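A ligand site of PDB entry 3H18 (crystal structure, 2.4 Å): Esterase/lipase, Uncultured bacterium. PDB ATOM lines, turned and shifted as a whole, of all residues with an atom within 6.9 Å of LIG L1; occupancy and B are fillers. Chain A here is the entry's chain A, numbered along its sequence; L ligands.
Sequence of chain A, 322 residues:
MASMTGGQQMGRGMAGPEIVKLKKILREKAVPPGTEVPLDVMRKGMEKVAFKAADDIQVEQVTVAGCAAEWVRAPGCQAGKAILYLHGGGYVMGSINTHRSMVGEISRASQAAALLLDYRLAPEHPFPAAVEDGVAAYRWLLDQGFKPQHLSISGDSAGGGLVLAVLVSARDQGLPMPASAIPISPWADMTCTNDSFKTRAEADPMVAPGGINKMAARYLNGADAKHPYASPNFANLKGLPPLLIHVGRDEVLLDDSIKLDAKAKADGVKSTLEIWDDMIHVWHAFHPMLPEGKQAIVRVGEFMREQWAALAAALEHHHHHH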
ATOM      1  N   MET A  42       4.003  -9.026  10.938  1.00  0.00           N
ATOM      2  CA  MET A  42       4.590  -7.750  10.499  1.00  0.00           C
ATOM      3  C   MET A  42       3.583  -6.562  10.652  1.00  0.00           C
ATOM      4  O   MET A  42       3.966  -5.501  11.199  1.00  0.00           O
ATOM      5  CB  MET A  42       5.050  -7.832   9.078  1.00  0.00           C
ATOM      6  CG  MET A  42       6.055  -8.937   8.726  1.00  0.00           C
ATOM      7  SD  MET A  42       6.310  -8.930   6.886  1.00  0.00           S
ATOM      8  CE  MET A  42       4.992  -9.936   6.202  1.00  0.00           C
ATOM      9  N   MET A  46       4.303  -3.335  13.123  1.00  0.00           N
ATOM     10  CA  MET A  46       4.210  -1.988  12.643  1.00  0.00           C
ATOM     11  C   MET A  46       3.221  -1.220  13.451  1.00  0.00           C
ATOM     12  O   MET A  46       3.451  -0.039  13.640  1.00  0.00           O
ATOM     13  CB  MET A  46       3.814  -1.945  11.189  1.00  0.00           C
ATOM     14  CG  MET A  46       4.863  -1.452  10.269  1.00  0.00           C
ATOM     15  SD  MET A  46       4.003  -0.988   8.768  1.00  0.00           S
ATOM     16  CE  MET A  46       4.249   0.761   8.653  1.00  0.00           C
ATOM     17  N   HIS A  87      -0.079   6.070   2.492  1.00  0.00           N
ATOM     18  CA  HIS A  87       0.926   5.458   3.386  1.00  0.00           C
ATOM     19  C   HIS A  87       1.705   4.266   2.781  1.00  0.00           C
ATOM     20  O   HIS A  87       1.239   3.656   1.817  1.00  0.00           O
ATOM     21  CB  HIS A  87       0.224   5.016   4.707  1.00  0.00           C
ATOM     22  CG  HIS A  87      -0.699   3.845   4.553  1.00  0.00           C
ATOM     23  ND1 HIS A  87      -0.244   2.544   4.464  1.00  0.00           N
ATOM     24  CD2 HIS A  87      -2.054   3.778   4.524  1.00  0.00           C
ATOM     25  CE1 HIS A  87      -1.287   1.727   4.400  1.00  0.00           C
ATOM     26  NE2 HIS A  87      -2.397   2.448   4.362  1.00  0.00           N
ATOM     27  N   GLY A  88       2.914   3.997   3.305  1.00  0.00           N
ATOM     28  CA  GLY A  88       3.735   2.849   2.842  1.00  0.00           C
ATOM     29  C   GLY A  88       3.346   1.583   3.593  1.00  0.00           C
ATOM     30  O   GLY A  88       2.445   1.601   4.399  1.00  0.00           O
ATOM     31  N   GLY A  89       3.991   0.471   3.248  1.00  0.00           N
ATOM     32  CA  GLY A  89       3.684  -0.769   3.855  1.00  0.00           C
ATOM     33  C   GLY A  89       3.628  -1.838   2.814  1.00  0.00           C
ATOM     34  O   GLY A  89       3.009  -2.890   3.057  1.00  0.00           O
ATOM     35  N   GLY A  90       4.201  -1.575   1.661  1.00  0.00           N
ATOM     36  CA  GLY A  90       4.527  -2.697   0.714  1.00  0.00           C
ATOM     37  C   GLY A  90       3.207  -3.111   0.049  1.00  0.00           C
ATOM     38  O   GLY A  90       3.141  -4.167  -0.647  1.00  0.00           O
ATOM     39  N   TYR A  91       2.131  -2.315   0.288  1.00  0.00           N
ATOM     40  CA  TYR A  91       0.796  -2.668  -0.270  1.00  0.00           C
ATOM     41  C   TYR A  91       0.058  -3.748   0.538  1.00  0.00           C
ATOM     42  O   TYR A  91      -1.054  -4.109   0.140  1.00  0.00           O
ATOM     43  CB  TYR A  91       0.842  -3.103  -1.784  1.00  0.00           C
ATOM     44  CG  TYR A  91       1.016  -1.946  -2.760  1.00  0.00           C
ATOM     45  CD1 TYR A  91       2.140  -1.817  -3.452  1.00  0.00           C
ATOM     46  CD2 TYR A  91       0.078  -0.936  -2.900  1.00  0.00           C
ATOM     47  CE1 TYR A  91       2.352  -0.749  -4.342  1.00  0.00           C
ATOM     48  CE2 TYR A  91       0.301   0.134  -3.835  1.00  0.00           C
ATOM     49  CZ  TYR A  91       1.459   0.141  -4.547  1.00  0.00           C
ATOM     50  OH  TYR A  91       1.862   1.095  -5.452  1.00  0.00           O
ATOM     51  N   VAL A  92       0.679  -4.203   1.654  1.00  0.00           N
ATOM     52  CA  VAL A  92       0.205  -5.361   2.433  1.00  0.00           C
ATOM     53  C   VAL A  92      -0.014  -4.964   3.905  1.00  0.00           C
ATOM     54  O   VAL A  92      -0.670  -5.656   4.625  1.00  0.00           O
ATOM     55  CB  VAL A  92       1.144  -6.723   2.323  1.00  0.00           C
ATOM     56  CG1 VAL A  92       1.289  -7.283   0.873  1.00  0.00           C
ATOM     57  CG2 VAL A  92       2.523  -6.505   2.962  1.00  0.00           C
ATOM     58  N   MET A  93       0.559  -3.867   4.340  1.00  0.00           N
ATOM     59  CA  MET A  93       0.423  -3.375   5.707  1.00  0.00           C
ATOM     60  C   MET A  93       0.500  -1.842   5.862  1.00  0.00           C
ATOM     61  O   MET A  93       0.452  -1.112   4.841  1.00  0.00           O
ATOM     62  CB  MET A  93       1.531  -3.990   6.520  1.00  0.00           C
ATOM     63  CG  MET A  93       2.879  -3.683   6.032  1.00  0.00           C
ATOM     64  SD  MET A  93       3.917  -4.671   7.102  1.00  0.00           S
ATOM     65  CE  MET A  93       5.446  -4.408   6.258  1.00  0.00           C
ATOM     66  N   TYR A 119      -6.610   2.723   2.542  1.00  0.00           N
ATOM     67  CA  TYR A 119      -6.975   2.023   1.324  1.00  0.00           C
ATOM     68  C   TYR A 119      -6.790   0.495   1.465  1.00  0.00           C
ATOM     69  O   TYR A 119      -6.091   0.035   2.432  1.00  0.00           O
ATOM     70  CB  TYR A 119      -6.068   2.583   0.179  1.00  0.00           C
ATOM     71  CG  TYR A 119      -4.565   2.269   0.337  1.00  0.00           C
ATOM     72  CD1 TYR A 119      -4.051   0.976   0.046  1.00  0.00           C
ATOM     73  CD2 TYR A 119      -3.683   3.276   0.781  1.00  0.00           C
ATOM     74  CE1 TYR A 119      -2.625   0.712   0.120  1.00  0.00           C
ATOM     75  CE2 TYR A 119      -2.326   3.091   0.853  1.00  0.00           C
ATOM     76  CZ  TYR A 119      -1.751   1.805   0.537  1.00  0.00           C
ATOM     77  OH  TYR A 119      -0.337   1.670   0.670  1.00  0.00           O
ATOM     78  N   ASP A 156       4.403   7.599   0.813  1.00  0.00           N
ATOM     79  CA  ASP A 156       5.703   6.984   1.059  1.00  0.00           C
ATOM     80  C   ASP A 156       5.766   5.566   0.587  1.00  0.00           C
ATOM     81  O   ASP A 156       4.870   4.744   0.844  1.00  0.00           O
ATOM     82  CB  ASP A 156       6.184   7.068   2.498  1.00  0.00           C
ATOM     83  CG  ASP A 156       5.159   6.546   3.509  1.00  0.00           C
ATOM     84  OD1 ASP A 156       5.440   5.510   4.120  1.00  0.00           O
ATOM     85  OD2 ASP A 156       4.064   7.171   3.697  1.00  0.00           O
ATOM     86  N   SER A 157       6.850   5.277  -0.130  1.00  0.00           N
ATOM     87  CA  SER A 157       7.204   3.937  -0.401  1.00  0.00           C
ATOM     88  C   SER A 157       6.167   3.338  -1.398  1.00  0.00           C
ATOM     89  O   SER A 157       6.061   3.872  -2.527  1.00  0.00           O
ATOM     90  CB  SER A 157       7.301   3.236   0.913  1.00  0.00           C
ATOM     91  OG  SER A 157       7.960   2.001   0.738  1.00  0.00           O
ATOM     92  N   ALA A 158       5.461   2.236  -1.031  1.00  0.00           N
ATOM     93  CA  ALA A 158       4.386   1.693  -1.847  1.00  0.00           C
ATOM     94  C   ALA A 158       3.416   2.848  -2.128  1.00  0.00           C
ATOM     95  O   ALA A 158       2.829   2.955  -3.190  1.00  0.00           O
ATOM     96  CB  ALA A 158       3.614   0.563  -1.030  1.00  0.00           C
ATOM     97  N   GLY A 159       3.170   3.672  -1.102  1.00  0.00           N
ATOM     98  CA  GLY A 159       2.207   4.713  -1.234  1.00  0.00           C
ATOM     99  C   GLY A 159       2.721   5.812  -2.116  1.00  0.00           C
ATOM    100  O   GLY A 159       1.936   6.545  -2.671  1.00  0.00           O
ATOM    101  N   SER A 185      10.581   8.265  -0.953  1.00  0.00           N
ATOM    102  CA  SER A 185      11.073   6.895  -1.143  1.00  0.00           C
ATOM    103  C   SER A 185      10.127   5.939  -1.981  1.00  0.00           C
ATOM    104  O   SER A 185       9.909   4.756  -1.613  1.00  0.00           O
ATOM    105  CB  SER A 185      11.455   6.254   0.194  1.00  0.00           C
ATOM    106  OG  SER A 185      12.398   7.054   0.885  1.00  0.00           O
ATOM    107  N   PRO A 186       9.636   6.424  -3.169  1.00  0.00           N
ATOM    108  CA  PRO A 186       8.636   5.687  -3.948  1.00  0.00           C
ATOM    109  C   PRO A 186       9.043   4.246  -4.285  1.00  0.00           C
ATOM    110  O   PRO A 186      10.227   4.007  -4.555  1.00  0.00           O
ATOM    111  CB  PRO A 186       8.551   6.481  -5.262  1.00  0.00           C
ATOM    112  CG  PRO A 186       9.766   7.320  -5.290  1.00  0.00           C
ATOM    113  CD  PRO A 186      10.073   7.658  -3.875  1.00  0.00           C
ATOM    114  N   TRP A 187       8.090   3.303  -4.227  1.00  0.00           N
ATOM    115  CA  TRP A 187       8.302   1.998  -4.815  1.00  0.00           C
ATOM    116  C   TRP A 187       7.477   1.952  -6.089  1.00  0.00           C
ATOM    117  O   TRP A 187       6.247   1.793  -6.059  1.00  0.00           O
ATOM    118  CB  TRP A 187       8.077   0.853  -3.803  1.00  0.00           C
ATOM    119  CG  TRP A 187       8.185  -0.509  -4.378  1.00  0.00           C
ATOM    120  CD1 TRP A 187       9.059  -0.969  -5.382  1.00  0.00           C
ATOM    121  CD2 TRP A 187       7.440  -1.675  -3.951  1.00  0.00           C
ATOM    122  NE1 TRP A 187       8.848  -2.324  -5.621  1.00  0.00           N
ATOM    123  CE2 TRP A 187       7.871  -2.786  -4.765  1.00  0.00           C
ATOM    124  CE3 TRP A 187       6.484  -1.899  -2.927  1.00  0.00           C
ATOM    125  CZ2 TRP A 187       7.360  -4.119  -4.571  1.00  0.00           C
ATOM    126  CZ3 TRP A 187       5.966  -3.235  -2.775  1.00  0.00           C
ATOM    127  CH2 TRP A 187       6.387  -4.295  -3.641  1.00  0.00           C
ATOM    128  N   MET A 206      17.372  -1.741   6.723  1.00  0.00           N
ATOM    129  CA  MET A 206      15.935  -1.505   6.652  1.00  0.00           C
ATOM    130  C   MET A 206      15.184  -1.926   5.341  1.00  0.00           C
ATOM    131  O   MET A 206      14.401  -2.875   5.316  1.00  0.00           O
ATOM    132  CB  MET A 206      15.779   0.008   6.831  1.00  0.00           C
ATOM    133  CG  MET A 206      14.378   0.546   6.621  1.00  0.00           C
ATOM    134  SD  MET A 206      14.230   1.716   7.967  1.00  0.00           S
ATOM    135  CE  MET A 206      14.881   0.621   9.291  1.00  0.00           C
ATOM    136  N   GLY A 211      12.467  -9.848   1.079  1.00  0.00           N
ATOM    137  CA  GLY A 211      11.193  -9.598   1.793  1.00  0.00           C
ATOM    138  C   GLY A 211      10.198  -8.771   0.941  1.00  0.00           C
ATOM    139  O   GLY A 211       8.991  -9.026   0.959  1.00  0.00           O
ATOM    140  N   ILE A 212      10.726  -7.788   0.201  1.00  0.00           N
ATOM    141  CA  ILE A 212       9.950  -6.874  -0.683  1.00  0.00           C
ATOM    142  C   ILE A 212       9.452  -7.585  -1.951  1.00  0.00           C
ATOM    143  O   ILE A 212       8.547  -7.118  -2.592  1.00  0.00           O
ATOM    144  CB  ILE A 212      10.831  -5.711  -1.167  1.00  0.00           C
ATOM    145  CG1 ILE A 212      10.023  -4.676  -1.953  1.00  0.00           C
ATOM    146  CG2 ILE A 212      12.140  -6.336  -1.869  1.00  0.00           C
ATOM    147  CD1 ILE A 212      10.343  -3.167  -1.619  1.00  0.00           C
ATOM    148  N   MET A 215       6.101  -9.123  -1.201  1.00  0.00           N
ATOM    149  CA  MET A 215       5.064  -8.156  -1.280  1.00  0.00           C
ATOM    150  C   MET A 215       4.678  -7.800  -2.691  1.00  0.00           C
ATOM    151  O   MET A 215       3.526  -7.475  -2.941  1.00  0.00           O
ATOM    152  CB  MET A 215       5.404  -6.918  -0.473  1.00  0.00           C
ATOM    153  CG  MET A 215       5.057  -7.152   0.980  1.00  0.00           C
ATOM    154  SD  MET A 215       6.245  -6.125   1.719  1.00  0.00           S
ATOM    155  CE  MET A 215       6.900  -7.330   2.934  1.00  0.00           C
ATOM    156  N   LEU A 253      15.902   1.229  -2.473  1.00  0.00           N
ATOM    157  CA  LEU A 253      15.005   1.661  -3.465  1.00  0.00           C
ATOM    158  C   LEU A 253      15.491   2.934  -4.139  1.00  0.00           C
ATOM    159  O   LEU A 253      14.635   3.621  -4.752  1.00  0.00           O
ATOM    160  CB  LEU A 253      13.666   2.070  -2.781  1.00  0.00           C
ATOM    161  CG  LEU A 253      12.645   0.998  -2.402  1.00  0.00           C
ATOM    162  CD1 LEU A 253      11.513   1.685  -1.639  1.00  0.00           C
ATOM    163  CD2 LEU A 253      12.209   0.287  -3.666  1.00  0.00           C
ATOM    164  N   HIS A 281      15.330   4.950   4.269  1.00  0.00           N
ATOM    165  CA  HIS A 281      14.006   4.852   3.815  1.00  0.00           C
ATOM    166  C   HIS A 281      13.108   5.675   4.641  1.00  0.00           C
ATOM    167  O   HIS A 281      13.007   5.471   5.846  1.00  0.00           O
ATOM    168  CB  HIS A 281      13.577   3.399   3.882  1.00  0.00           C
ATOM    169  CG  HIS A 281      12.255   3.150   3.243  1.00  0.00           C
ATOM    170  ND1 HIS A 281      12.029   3.381   1.901  1.00  0.00           N
ATOM    171  CD2 HIS A 281      11.087   2.705   3.755  1.00  0.00           C
ATOM    172  CE1 HIS A 281      10.762   3.133   1.620  1.00  0.00           C
ATOM    173  NE2 HIS A 281      10.162   2.769   2.741  1.00  0.00           N
ATOM    174  N   VAL A 282      12.416   6.608   3.987  1.00  0.00           N
ATOM    175  CA  VAL A 282      11.447   7.416   4.653  1.00  0.00           C
ATOM    176  C   VAL A 282      11.973   7.933   6.000  1.00  0.00           C
ATOM    177  O   VAL A 282      11.324   7.846   7.047  1.00  0.00           O
ATOM    178  CB  VAL A 282      10.115   6.674   4.779  1.00  0.00           C
ATOM    179  CG1 VAL A 282       9.045   7.595   5.281  1.00  0.00           C
ATOM    180  CG2 VAL A 282       9.711   6.100   3.423  1.00  0.00           C
HETATM  181  C1  LIG L   1       8.898  -0.036   2.042  1.00  0.00           C
HETATM  182  S1  LIG L   1       7.759   0.530   0.907  1.00  0.00           S
HETATM  183  C2  LIG L   1       8.297  -1.087   2.884  1.00  0.00           C
HETATM  184  C3  LIG L   1       7.735  -0.655   4.141  1.00  0.00           C
HETATM  185  C4  LIG L   1       7.182  -1.612   5.020  1.00  0.00           C
HETATM  186  C5  LIG L   1       7.280  -2.992   4.534  1.00  0.00           C
HETATM  187  C6  LIG L   1       7.890  -3.427   3.298  1.00  0.00           C
HETATM  188  C7  LIG L   1       8.403  -2.442   2.445  1.00  0.00           C
HETATM  189  O1  LIG L   1       7.767  -0.871  -0.030  1.00  0.00           O
HETATM  190  O2  LIG L   1       6.164   0.232   1.347  1.00  0.00           O
HETATM  191  C1  LG2 L   2       7.342   2.806   6.972  1.00  0.00           C
HETATM  192  S1  LG2 L   2       7.127   2.235   5.313  1.00  0.00           S
HETATM  193  C2  LG2 L   2       6.755   3.976   7.706  1.00  0.00           C
HETATM  194  C3  LG2 L   2       6.783   5.245   7.211  1.00  0.00           C
HETATM  195  C4  LG2 L   2       6.221   6.291   7.971  1.00  0.00           C
HETATM  196  C5  LG2 L   2       5.696   6.001   9.218  1.00  0.00           C
HETATM  197  C6  LG2 L   2       5.735   4.665   9.721  1.00  0.00           C
HETATM  198  C7  LG2 L   2       6.268   3.676   8.984  1.00  0.00           C
HETATM  199  O1  LG2 L   2       6.039   0.953   5.608  1.00  0.00           O
HETATM  200  O2  LG2 L   2       6.593   3.304   4.131  1.00  0.00           O
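NE2 of His 281 lies within hydrogen-bond range of OG of Ser 157 (3.1 Å).
The backbone carbonyl oxygen (O) of Ser 157 sits at hydrogen-bond distance from the backbone NH (N) of Trp 187.
The backbone NH of Ser 157 sits close to the backbone carbonyl oxygen of Ser 185, 3.4 Å away.
The backbone carbonyl oxygen (O) of Ala 158 lies within hydrogen-bond range of the side-chain hydroxyl (OH) of Tyr 91.
The side-chain carboxylate (OD1) of Asp 156 is in hydrogen-bond range of the backbone NH (N) of Gly 88, at 3.1 Å.
A sulfur (S1) of LIG L1 is covalently linked to the side-chain hydroxyl (OG) of Ser 157, 1.5 Å away.
O2 of LIG L1 lies within hydrogen-bond range of N of Gly 90.
O2 of LIG L1 is in hydrogen-bond range of N of Gly 89, at 2.9 Å.
O2 of LIG L1 is in hydrogen-bond range of N of Ala 158, 3.2 Å away.
O1 of LG2 L2 lies within hydrogen-bond range of N of Gly 89, 3.2 Å away.
The side-chain carboxylate of Asp 156 sits close to an oxygen (O2) of LG2 L2, 2.5 Å away.
A sulfur (S1) of LIG L1 lies close to a ring nitrogen (NE2) of His 281 (3.8 Å).
Merely in contact with LIG L1: Met 93, Trp 187, Met 215, Ile 212 and Gly 88.
Hydrophobic or aromatic side chains within 4 Å of LIG L1: Met 93, Ala 158, Trp 187, Ile 212, Met 215 and His 281.
Ten residues have an atom within 4 Å of LIG L1: Gly 88, Gly 89, Gly 90, Met 93, Ser 157, Ala 158, Trp 187, Ile 212, Met 215 and His 281.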
